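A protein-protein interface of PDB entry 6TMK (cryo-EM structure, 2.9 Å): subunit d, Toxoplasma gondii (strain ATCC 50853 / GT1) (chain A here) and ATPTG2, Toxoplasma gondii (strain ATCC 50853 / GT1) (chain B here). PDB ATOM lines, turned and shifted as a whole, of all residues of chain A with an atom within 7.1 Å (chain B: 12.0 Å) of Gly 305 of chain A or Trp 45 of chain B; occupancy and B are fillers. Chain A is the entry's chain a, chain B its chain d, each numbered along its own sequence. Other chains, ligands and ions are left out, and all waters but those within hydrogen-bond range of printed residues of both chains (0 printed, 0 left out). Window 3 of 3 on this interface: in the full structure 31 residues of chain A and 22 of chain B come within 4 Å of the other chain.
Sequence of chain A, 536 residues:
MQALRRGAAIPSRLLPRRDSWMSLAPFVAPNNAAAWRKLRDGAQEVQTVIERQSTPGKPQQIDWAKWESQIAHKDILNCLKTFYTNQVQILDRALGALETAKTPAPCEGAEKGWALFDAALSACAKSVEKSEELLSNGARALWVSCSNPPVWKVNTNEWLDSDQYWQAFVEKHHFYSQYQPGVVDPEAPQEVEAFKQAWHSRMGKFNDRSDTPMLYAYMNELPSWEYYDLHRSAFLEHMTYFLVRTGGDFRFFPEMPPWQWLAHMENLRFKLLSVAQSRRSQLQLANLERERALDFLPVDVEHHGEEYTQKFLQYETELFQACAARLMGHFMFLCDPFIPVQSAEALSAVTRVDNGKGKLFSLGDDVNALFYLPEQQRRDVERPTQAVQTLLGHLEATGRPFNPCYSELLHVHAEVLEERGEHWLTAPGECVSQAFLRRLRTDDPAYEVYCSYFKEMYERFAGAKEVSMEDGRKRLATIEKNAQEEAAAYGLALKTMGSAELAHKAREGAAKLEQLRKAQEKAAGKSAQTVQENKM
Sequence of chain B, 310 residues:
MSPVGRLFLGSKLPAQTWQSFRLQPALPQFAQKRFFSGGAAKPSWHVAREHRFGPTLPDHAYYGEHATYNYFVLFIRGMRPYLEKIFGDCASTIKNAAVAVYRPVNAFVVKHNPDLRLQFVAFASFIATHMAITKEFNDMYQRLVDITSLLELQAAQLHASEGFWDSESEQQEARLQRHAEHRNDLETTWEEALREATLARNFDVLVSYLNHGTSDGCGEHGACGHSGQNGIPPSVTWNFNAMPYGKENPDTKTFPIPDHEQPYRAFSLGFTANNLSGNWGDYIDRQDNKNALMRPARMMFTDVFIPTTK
The backbone carbonyl oxygen of Leu 230 of chain A sits at hydrogen-bond distance from the backbone NH of Ser 44 of chain B (2.8 Å).
The guanidinium group (NH2) of Arg 52 of chain B lies within salt-bridge range of the side-chain carboxylate (OE1) of Glu 237 of chain A (3.8 Å).
O of His 46 of chain B sits at hydrogen-bond distance from OG of Ser 44 of chain B, at 2.8 Å.
The side-chain hydroxyl (OG) of Ser 233 of chain A lies within hydrogen-bond range of the side-chain carboxylate (OE2) of Glu 237 of chain A (2.8 Å).
The side-chain hydroxyl (OG1) of Thr 309 of chain A sits at hydrogen-bond distance from the backbone carbonyl oxygen (O) of Gly 305 of chain A (2.7 Å).
Among the printed residues, merely in contact across the chains: Leu 230 of chain A with Pro 43 of chain B (3.2 Å), His 231 of chain A with Ser 44 of chain B (3.8 Å), His 231 of chain A with His 46 of chain B (3.9 Å), His 231 of chain A with Val 47 of chain B (3.9 Å), His 231 of chain A with His 51 of chain B (3.96 Å), Arg 232 of chain A with Ser 44 of chain B (3.7 Å), Arg 232 of chain A with Trp 45 of chain B (3.9 Å), Ser 233 of chain A with Trp 45 of chain B (3.4 Å), Gly 305 of chain A with Trp 45 of chain B (3.9 Å), Glu 306 of chain A with Trp 45 of chain B (3.4 Å) and Thr 309 of chain A with Trp 45 of chain B (3.8 Å).
Gly 305 of chain A touches just one residue of chain B: Trp 45 (3.9 Å).
Of chain A, only Arg 232 (3.9 Å), Ser 233 (3.4 Å), Gly 305 (3.9 Å), Glu 306 (3.4 Å) and Thr 309 (3.8 Å) come within 4 Å of Trp 45 of chain B.
Ser 233 of chain A touches just one residue of chain B: Trp 45.
Of chain B, only Trp 45 (3.4 Å) comes within 4 Å of Glu 306 of chain A.
Glu 307 of chain A touches none of the printed residues of chain B.
No residue of chain B comes within 4 Å of Tyr 308 of chain A.
Thr 309 of chain A touches just one residue of chain B: Trp 45.
Printed residues of chain A within 4 Å of Val 47 of chain B: His 231 (3.9 Å).
Printed residues of chain B within 4 Å of Leu 230 of chain A: Pro 43 and Ser 44.
The nearest residue of chain A that does not touch Trp 45 of chain B is Leu 236 of chain A (4.2 Å).
The nearest printed residue of chain A that does not touch Ser 44 of chain B is Ser 233 of chain A (4.7 Å).
Of the 11 printed residues of chain B, 7 touch a printed residue of chain A.
Hydrophobic or aromatic side chains of chain B that line the printed part of chain A: Pro 43, Trp 45, Val 47 and His 51.
Of the 15 printed residues of chain A, 8 touch a printed residue of chain B.
Among the printed residues, Asp or Glu carboxylates within 4 Å of a Lys or Arg side-chain nitrogen of the other chain: Glu 237 of chain A with Arg 52 of chain B.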
ATOM      1  N   LEU A 230      10.884   9.262  -1.829  1.00  0.00           N
ATOM      2  CA  LEU A 230      10.580  10.683  -1.914  1.00  0.00           C
ATOM      3  C   LEU A 230       9.723  11.159  -0.753  1.00  0.00           C
ATOM      4  O   LEU A 230       9.888  12.292  -0.291  1.00  0.00           O
ATOM      5  CB  LEU A 230       9.872  10.986  -3.229  1.00  0.00           C
ATOM      6  CG  LEU A 230      10.667  10.718  -4.502  1.00  0.00           C
ATOM      7  CD1 LEU A 230       9.797  10.879  -5.719  1.00  0.00           C
ATOM      8  CD2 LEU A 230      11.839  11.642  -4.582  1.00  0.00           C
ATOM      9  N   HIS A 231       8.813  10.322  -0.270  1.00  0.00           N
ATOM     10  CA  HIS A 231       7.871  10.672   0.785  1.00  0.00           C
ATOM     11  C   HIS A 231       8.205   9.838   2.017  1.00  0.00           C
ATOM     12  O   HIS A 231       7.672   8.746   2.210  1.00  0.00           O
ATOM     13  CB  HIS A 231       6.453  10.434   0.320  1.00  0.00           C
ATOM     14  CG  HIS A 231       6.146  11.045  -1.010  1.00  0.00           C
ATOM     15  ND1 HIS A 231       6.064  12.406  -1.203  1.00  0.00           N
ATOM     16  CD2 HIS A 231       5.901  10.480  -2.214  1.00  0.00           C
ATOM     17  CE1 HIS A 231       5.782  12.652  -2.470  1.00  0.00           C
ATOM     18  NE2 HIS A 231       5.678  11.499  -3.104  1.00  0.00           N
ATOM     19  N   ARG A 232       9.097  10.367   2.853  1.00  0.00           N
ATOM     20  CA  ARG A 232       9.498   9.662   4.059  1.00  0.00           C
ATOM     21  C   ARG A 232       8.422   9.705   5.130  1.00  0.00           C
ATOM     22  O   ARG A 232       8.407   8.841   6.012  1.00  0.00           O
ATOM     23  CB  ARG A 232      10.791  10.261   4.601  1.00  0.00           C
ATOM     24  CG  ARG A 232      11.874  10.430   3.560  1.00  0.00           C
ATOM     25  CD  ARG A 232      12.164   9.130   2.857  1.00  0.00           C
ATOM     26  NE  ARG A 232      13.400   9.183   2.086  1.00  0.00           N
ATOM     27  CZ  ARG A 232      14.613   9.057   2.607  1.00  0.00           C
ATOM     28  NH1 ARG A 232      14.766   8.879   3.906  1.00  0.00           N
ATOM     29  NH2 ARG A 232      15.675   9.115   1.826  1.00  0.00           N
ATOM     30  N   SER A 233       7.524  10.688   5.075  1.00  0.00           N
ATOM     31  CA  SER A 233       6.414  10.730   6.017  1.00  0.00           C
ATOM     32  C   SER A 233       5.500   9.530   5.838  1.00  0.00           C
ATOM     33  O   SER A 233       4.999   8.966   6.817  1.00  0.00           O
ATOM     34  CB  SER A 233       5.633  12.026   5.831  1.00  0.00           C
ATOM     35  OG  SER A 233       4.444  12.022   6.600  1.00  0.00           O
ATOM     36  N   ALA A 234       5.272   9.124   4.590  1.00  0.00           N
ATOM     37  CA  ALA A 234       4.343   8.041   4.312  1.00  0.00           C
ATOM     38  C   ALA A 234       4.961   6.679   4.581  1.00  0.00           C
ATOM     39  O   ALA A 234       4.251   5.748   4.970  1.00  0.00           O
ATOM     40  CB  ALA A 234       3.872   8.128   2.866  1.00  0.00           C
ATOM     41  N   LEU A 236       6.918   5.987   7.040  1.00  0.00           N
ATOM     42  CA  LEU A 236       6.771   5.782   8.473  1.00  0.00           C
ATOM     43  C   LEU A 236       5.345   5.374   8.818  1.00  0.00           C
ATOM     44  O   LEU A 236       5.120   4.382   9.517  1.00  0.00           O
ATOM     45  CB  LEU A 236       7.170   7.057   9.206  1.00  0.00           C
ATOM     46  CG  LEU A 236       7.325   6.960  10.714  1.00  0.00           C
ATOM     47  CD1 LEU A 236       8.542   6.143  11.050  1.00  0.00           C
ATOM     48  CD2 LEU A 236       7.437   8.338  11.302  1.00  0.00           C
ATOM     49  N   GLU A 237       4.364   6.133   8.330  1.00  0.00           N
ATOM     50  CA  GLU A 237       2.971   5.840   8.640  1.00  0.00           C
ATOM     51  C   GLU A 237       2.562   4.475   8.104  1.00  0.00           C
ATOM     52  O   GLU A 237       1.934   3.679   8.809  1.00  0.00           O
ATOM     53  CB  GLU A 237       2.072   6.928   8.060  1.00  0.00           C
ATOM     54  CG  GLU A 237       2.254   8.279   8.705  1.00  0.00           C
ATOM     55  CD  GLU A 237       2.019   9.425   7.739  1.00  0.00           C
ATOM     56  OE1 GLU A 237       1.278   9.234   6.752  1.00  0.00           O
ATOM     57  OE2 GLU A 237       2.571  10.521   7.968  1.00  0.00           O
ATOM     58  N   HIS A 304       9.951  21.766  10.442  1.00  0.00           N
ATOM     59  CA  HIS A 304      10.634  20.487  10.289  1.00  0.00           C
ATOM     60  C   HIS A 304       9.972  19.431  11.165  1.00  0.00           C
ATOM     61  O   HIS A 304      10.197  19.383  12.373  1.00  0.00           O
ATOM     62  CB  HIS A 304      12.111  20.620  10.651  1.00  0.00           C
ATOM     63  CG  HIS A 304      12.788  21.787  10.002  1.00  0.00           C
ATOM     64  ND1 HIS A 304      13.455  21.686   8.800  1.00  0.00           N
ATOM     65  CD2 HIS A 304      12.901  23.079  10.389  1.00  0.00           C
ATOM     66  CE1 HIS A 304      13.950  22.867   8.475  1.00  0.00           C
ATOM     67  NE2 HIS A 304      13.628  23.729   9.422  1.00  0.00           N
ATOM     68  N   GLY A 305       9.152  18.583  10.542  1.00  0.00           N
ATOM     69  CA  GLY A 305       8.500  17.508  11.267  1.00  0.00           C
ATOM     70  C   GLY A 305       9.331  16.255  11.419  1.00  0.00           C
ATOM     71  O   GLY A 305       9.097  15.481  12.351  1.00  0.00           O
ATOM     72  N   GLU A 306      10.303  16.041  10.531  1.00  0.00           N
ATOM     73  CA  GLU A 306      11.115  14.832  10.602  1.00  0.00           C
ATOM     74  C   GLU A 306      11.930  14.793  11.887  1.00  0.00           C
ATOM     75  O   GLU A 306      11.960  13.773  12.587  1.00  0.00           O
ATOM     76  CB  GLU A 306      12.033  14.757   9.385  1.00  0.00           C
ATOM     77  CG  GLU A 306      12.834  13.474   9.296  1.00  0.00           C
ATOM     78  CD  GLU A 306      13.150  13.080   7.869  1.00  0.00           C
ATOM     79  OE1 GLU A 306      13.161  13.967   6.990  1.00  0.00           O
ATOM     80  OE2 GLU A 306      13.388  11.879   7.623  1.00  0.00           O
ATOM     81  N   GLU A 307      12.595  15.899  12.216  1.00  0.00           N
ATOM     82  CA  GLU A 307      13.403  15.943  13.428  1.00  0.00           C
ATOM     83  C   GLU A 307      12.537  15.776  14.668  1.00  0.00           C
ATOM     84  O   GLU A 307      12.919  15.074  15.612  1.00  0.00           O
ATOM     85  CB  GLU A 307      14.174  17.256  13.485  1.00  0.00           C
ATOM     86  CG  GLU A 307      15.164  17.427  12.354  1.00  0.00           C
ATOM     87  CD  GLU A 307      15.503  18.882  12.092  1.00  0.00           C
ATOM     88  OE1 GLU A 307      15.861  19.213  10.942  1.00  0.00           O
ATOM     89  OE2 GLU A 307      15.407  19.695  13.035  1.00  0.00           O
ATOM     90  N   TYR A 308      11.366  16.412  14.684  1.00  0.00           N
ATOM     91  CA  TYR A 308      10.488  16.304  15.842  1.00  0.00           C
ATOM     92  C   TYR A 308       9.987  14.879  16.018  1.00  0.00           C
ATOM     93  O   TYR A 308       9.957  14.362  17.140  1.00  0.00           O
ATOM     94  CB  TYR A 308       9.310  17.263  15.696  1.00  0.00           C
ATOM     95  CG  TYR A 308       9.628  18.690  16.071  1.00  0.00           C
ATOM     96  CD1 TYR A 308       8.935  19.331  17.088  1.00  0.00           C
ATOM     97  CD2 TYR A 308      10.616  19.398  15.405  1.00  0.00           C
ATOM     98  CE1 TYR A 308       9.219  20.635  17.430  1.00  0.00           C
ATOM     99  CE2 TYR A 308      10.908  20.702  15.741  1.00  0.00           C
ATOM    100  CZ  TYR A 308      10.206  21.317  16.754  1.00  0.00           C
ATOM    101  OH  TYR A 308      10.495  22.618  17.091  1.00  0.00           O
ATOM    102  N   THR A 309       9.596  14.226  14.922  1.00  0.00           N
ATOM    103  CA  THR A 309       9.150  12.842  15.009  1.00  0.00           C
ATOM    104  C   THR A 309      10.276  11.933  15.477  1.00  0.00           C
ATOM    105  O   THR A 309      10.061  11.032  16.299  1.00  0.00           O
ATOM    106  CB  THR A 309       8.623  12.383  13.652  1.00  0.00           C
ATOM    107  OG1 THR A 309       7.671  13.333  13.160  1.00  0.00           O
ATOM    108  CG2 THR A 309       7.964  11.029  13.770  1.00  0.00           C
ATOM    109  N   GLN A 310      11.485  12.156  14.967  1.00  0.00           N
ATOM    110  CA  GLN A 310      12.626  11.351  15.384  1.00  0.00           C
ATOM    111  C   GLN A 310      12.877  11.503  16.877  1.00  0.00           C
ATOM    112  O   GLN A 310      13.061  10.513  17.595  1.00  0.00           O
ATOM    113  CB  GLN A 310      13.857  11.761  14.581  1.00  0.00           C
ATOM    114  CG  GLN A 310      14.895  10.673  14.436  1.00  0.00           C
ATOM    115  CD  GLN A 310      14.545   9.668  13.364  1.00  0.00           C
ATOM    116  OE1 GLN A 310      13.727   9.937  12.485  1.00  0.00           O
ATOM    117  NE2 GLN A 310      15.165   8.500  13.431  1.00  0.00           N
ATOM    118  N   LYS A 311      12.881  12.745  17.361  1.00  0.00           N
ATOM    119  CA  LYS A 311      13.095  12.998  18.782  1.00  0.00           C
ATOM    120  C   LYS A 311      12.011  12.339  19.620  1.00  0.00           C
ATOM    121  O   LYS A 311      12.295  11.701  20.641  1.00  0.00           O
ATOM    122  CB  LYS A 311      13.128  14.501  19.039  1.00  0.00           C
ATOM    123  CG  LYS A 311      14.410  15.174  18.597  1.00  0.00           C
ATOM    124  CD  LYS A 311      14.501  16.591  19.136  1.00  0.00           C
ATOM    125  CE  LYS A 311      13.376  17.459  18.607  1.00  0.00           C
ATOM    126  NZ  LYS A 311      13.700  18.907  18.677  1.00  0.00           N
ATOM    127  N   ALA B  41      11.670  15.113  -7.146  1.00  0.00           N
ATOM    128  CA  ALA B  41      13.071  14.842  -7.443  1.00  0.00           C
ATOM    129  C   ALA B  41      13.888  14.766  -6.161  1.00  0.00           C
ATOM    130  O   ALA B  41      14.884  14.047  -6.086  1.00  0.00           O
ATOM    131  CB  ALA B  41      13.636  15.912  -8.360  1.00  0.00           C
ATOM    132  N   LYS B  42      13.455  15.517  -5.154  1.00  0.00           N
ATOM    133  CA  LYS B  42      14.110  15.572  -3.863  1.00  0.00           C
ATOM    134  C   LYS B  42      13.148  15.097  -2.784  1.00  0.00           C
ATOM    135  O   LYS B  42      11.980  15.512  -2.780  1.00  0.00           O
ATOM    136  CB  LYS B  42      14.576  16.998  -3.554  1.00  0.00           C
ATOM    137  CG  LYS B  42      16.087  17.158  -3.488  1.00  0.00           C
ATOM    138  CD  LYS B  42      16.532  18.491  -4.066  1.00  0.00           C
ATOM    139  CE  LYS B  42      16.539  19.582  -3.009  1.00  0.00           C
ATOM    140  NZ  LYS B  42      17.785  19.560  -2.196  1.00  0.00           N
ATOM    141  N   PRO B  43      13.580  14.240  -1.861  1.00  0.00           N
ATOM    142  CA  PRO B  43      12.652  13.758  -0.834  1.00  0.00           C
ATOM    143  C   PRO B  43      12.213  14.875   0.096  1.00  0.00           C
ATOM    144  O   PRO B  43      12.998  15.749   0.471  1.00  0.00           O
ATOM    145  CB  PRO B  43      13.465  12.692  -0.091  1.00  0.00           C
ATOM    146  CG  PRO B  43      14.875  13.037  -0.338  1.00  0.00           C
ATOM    147  CD  PRO B  43      14.938  13.708  -1.675  1.00  0.00           C
ATOM    148  N   SER B  44      10.936  14.830   0.465  1.00  0.00           N
ATOM    149  CA  SER B  44      10.331  15.819   1.340  1.00  0.00           C
ATOM    150  C   SER B  44       9.429  15.130   2.352  1.00  0.00           C
ATOM    151  O   SER B  44       8.952  14.014   2.133  1.00  0.00           O
ATOM    152  CB  SER B  44       9.528  16.851   0.541  1.00  0.00           C
ATOM    153  OG  SER B  44       8.213  16.387   0.291  1.00  0.00           O
ATOM    154  N   TRP B  45       9.212  15.808   3.473  1.00  0.00           N
ATOM    155  CA  TRP B  45       8.366  15.299   4.539  1.00  0.00           C
ATOM    156  C   TRP B  45       6.903  15.671   4.328  1.00  0.00           C
ATOM    157  O   TRP B  45       6.066  15.383   5.188  1.00  0.00           O
ATOM    158  CB  TRP B  45       8.845  15.831   5.892  1.00  0.00           C
ATOM    159  CG  TRP B  45       8.270  15.097   7.056  1.00  0.00           C
ATOM    160  CD1 TRP B  45       7.190  15.464   7.799  1.00  0.00           C
ATOM    161  CD2 TRP B  45       8.733  13.861   7.606  1.00  0.00           C
ATOM    162  NE1 TRP B  45       6.953  14.536   8.779  1.00  0.00           N
ATOM    163  CE2 TRP B  45       7.889  13.542   8.683  1.00  0.00           C
ATOM    164  CE3 TRP B  45       9.783  12.996   7.294  1.00  0.00           C
ATOM    165  CZ2 TRP B  45       8.058  12.396   9.446  1.00  0.00           C
ATOM    166  CZ3 TRP B  45       9.948  11.859   8.056  1.00  0.00           C
ATOM    167  CH2 TRP B  45       9.092  11.570   9.118  1.00  0.00           C
ATOM    168  N   HIS B  46       6.580  16.282   3.192  1.00  0.00           N
ATOM    169  CA  HIS B  46       5.227  16.700   2.854  1.00  0.00           C
ATOM    170  C   HIS B  46       4.755  15.923   1.635  1.00  0.00           C
ATOM    171  O   HIS B  46       5.499  15.783   0.659  1.00  0.00           O
ATOM    172  CB  HIS B  46       5.171  18.203   2.575  1.00  0.00           C
ATOM    173  CG  HIS B  46       3.839  18.679   2.087  1.00  0.00           C
ATOM    174  ND1 HIS B  46       3.640  19.153   0.808  1.00  0.00           N
ATOM    175  CD2 HIS B  46       2.639  18.760   2.709  1.00  0.00           C
ATOM    176  CE1 HIS B  46       2.374  19.501   0.662  1.00  0.00           C
ATOM    177  NE2 HIS B  46       1.745  19.271   1.800  1.00  0.00           N
ATOM    178  N   VAL B  47       3.527  15.415   1.696  1.00  0.00           N
ATOM    179  CA  VAL B  47       2.933  14.644   0.612  1.00  0.00           C
ATOM    180  C   VAL B  47       1.856  15.491  -0.049  1.00  0.00           C
ATOM    181  O   VAL B  47       0.989  16.052   0.631  1.00  0.00           O
ATOM    182  CB  VAL B  47       2.351  13.314   1.116  1.00  0.00           C
ATOM    183  CG1 VAL B  47       1.716  12.554  -0.023  1.00  0.00           C
ATOM    184  CG2 VAL B  47       3.432  12.483   1.763  1.00  0.00           C
ATOM    185  N   ALA B  48       1.913  15.575  -1.372  1.00  0.00           N
ATOM    186  CA  ALA B  48       0.981  16.380  -2.146  1.00  0.00           C
ATOM    187  C   ALA B  48      -0.399  15.727  -2.139  1.00  0.00           C
ATOM    188  O   ALA B  48      -0.651  14.734  -1.454  1.00  0.00           O
ATOM    189  CB  ALA B  48       1.509  16.571  -3.562  1.00  0.00           C
ATOM    190  N   ARG B  49      -1.317  16.302  -2.916  1.00  0.00           N
ATOM    191  CA  ARG B  49      -2.665  15.759  -3.022  1.00  0.00           C
ATOM    192  C   ARG B  49      -2.683  14.507  -3.892  1.00  0.00           C
ATOM    193  O   ARG B  49      -3.157  13.449  -3.463  1.00  0.00           O
ATOM    194  CB  ARG B  49      -3.595  16.825  -3.613  1.00  0.00           C
ATOM    195  CG  ARG B  49      -5.010  16.362  -3.940  1.00  0.00           C
ATOM    196  CD  ARG B  49      -5.787  15.983  -2.700  1.00  0.00           C
ATOM    197  NE  ARG B  49      -6.528  17.128  -2.179  1.00  0.00           N
ATOM    198  CZ  ARG B  49      -6.885  17.284  -0.907  1.00  0.00           C
ATOM    199  NH1 ARG B  49      -6.569  16.368  -0.002  1.00  0.00           N
ATOM    200  NH2 ARG B  49      -7.561  18.363  -0.540  1.00  0.00           N
ATOM    201  N   HIS B  51      -0.439  12.458  -4.679  1.00  0.00           N
ATOM    202  CA  HIS B  51       0.318  11.364  -4.094  1.00  0.00           C
ATOM    203  C   HIS B  51      -0.166  11.004  -2.700  1.00  0.00           C
ATOM    204  O   HIS B  51       0.567  10.361  -1.943  1.00  0.00           O
ATOM    205  CB  HIS B  51       1.802  11.714  -4.052  1.00  0.00           C
ATOM    206  CG  HIS B  51       2.405  11.965  -5.396  1.00  0.00           C
ATOM    207  ND1 HIS B  51       2.204  11.125  -6.469  1.00  0.00           N
ATOM    208  CD2 HIS B  51       3.214  12.955  -5.840  1.00  0.00           C
ATOM    209  CE1 HIS B  51       2.858  11.590  -7.518  1.00  0.00           C
ATOM    210  NE2 HIS B  51       3.477  12.701  -7.163  1.00  0.00           N
ATOM    211  N   ARG B  52      -1.384  11.407  -2.342  1.00  0.00           N
ATOM    212  CA  ARG B  52      -1.857  11.152  -0.989  1.00  0.00           C
ATOM    213  C   ARG B  52      -2.103   9.669  -0.759  1.00  0.00           C
ATOM    214  O   ARG B  52      -1.772   9.136   0.305  1.00  0.00           O
ATOM    215  CB  ARG B  52      -3.133  11.950  -0.727  1.00  0.00           C
ATOM    216  CG  ARG B  52      -3.680  11.814   0.681  1.00  0.00           C
ATOM    217  CD  ARG B  52      -2.705  12.339   1.708  1.00  0.00           C
ATOM    218  NE  ARG B  52      -1.776  11.303   2.144  1.00  0.00           N
ATOM    219  CZ  ARG B  52      -0.808  11.496   3.032  1.00  0.00           C
ATOM    220  NH1 ARG B  52      -0.641  12.686   3.587  1.00  0.00           N
ATOM    221  NH2 ARG B  52      -0.011  10.495   3.368  1.00  0.00           N
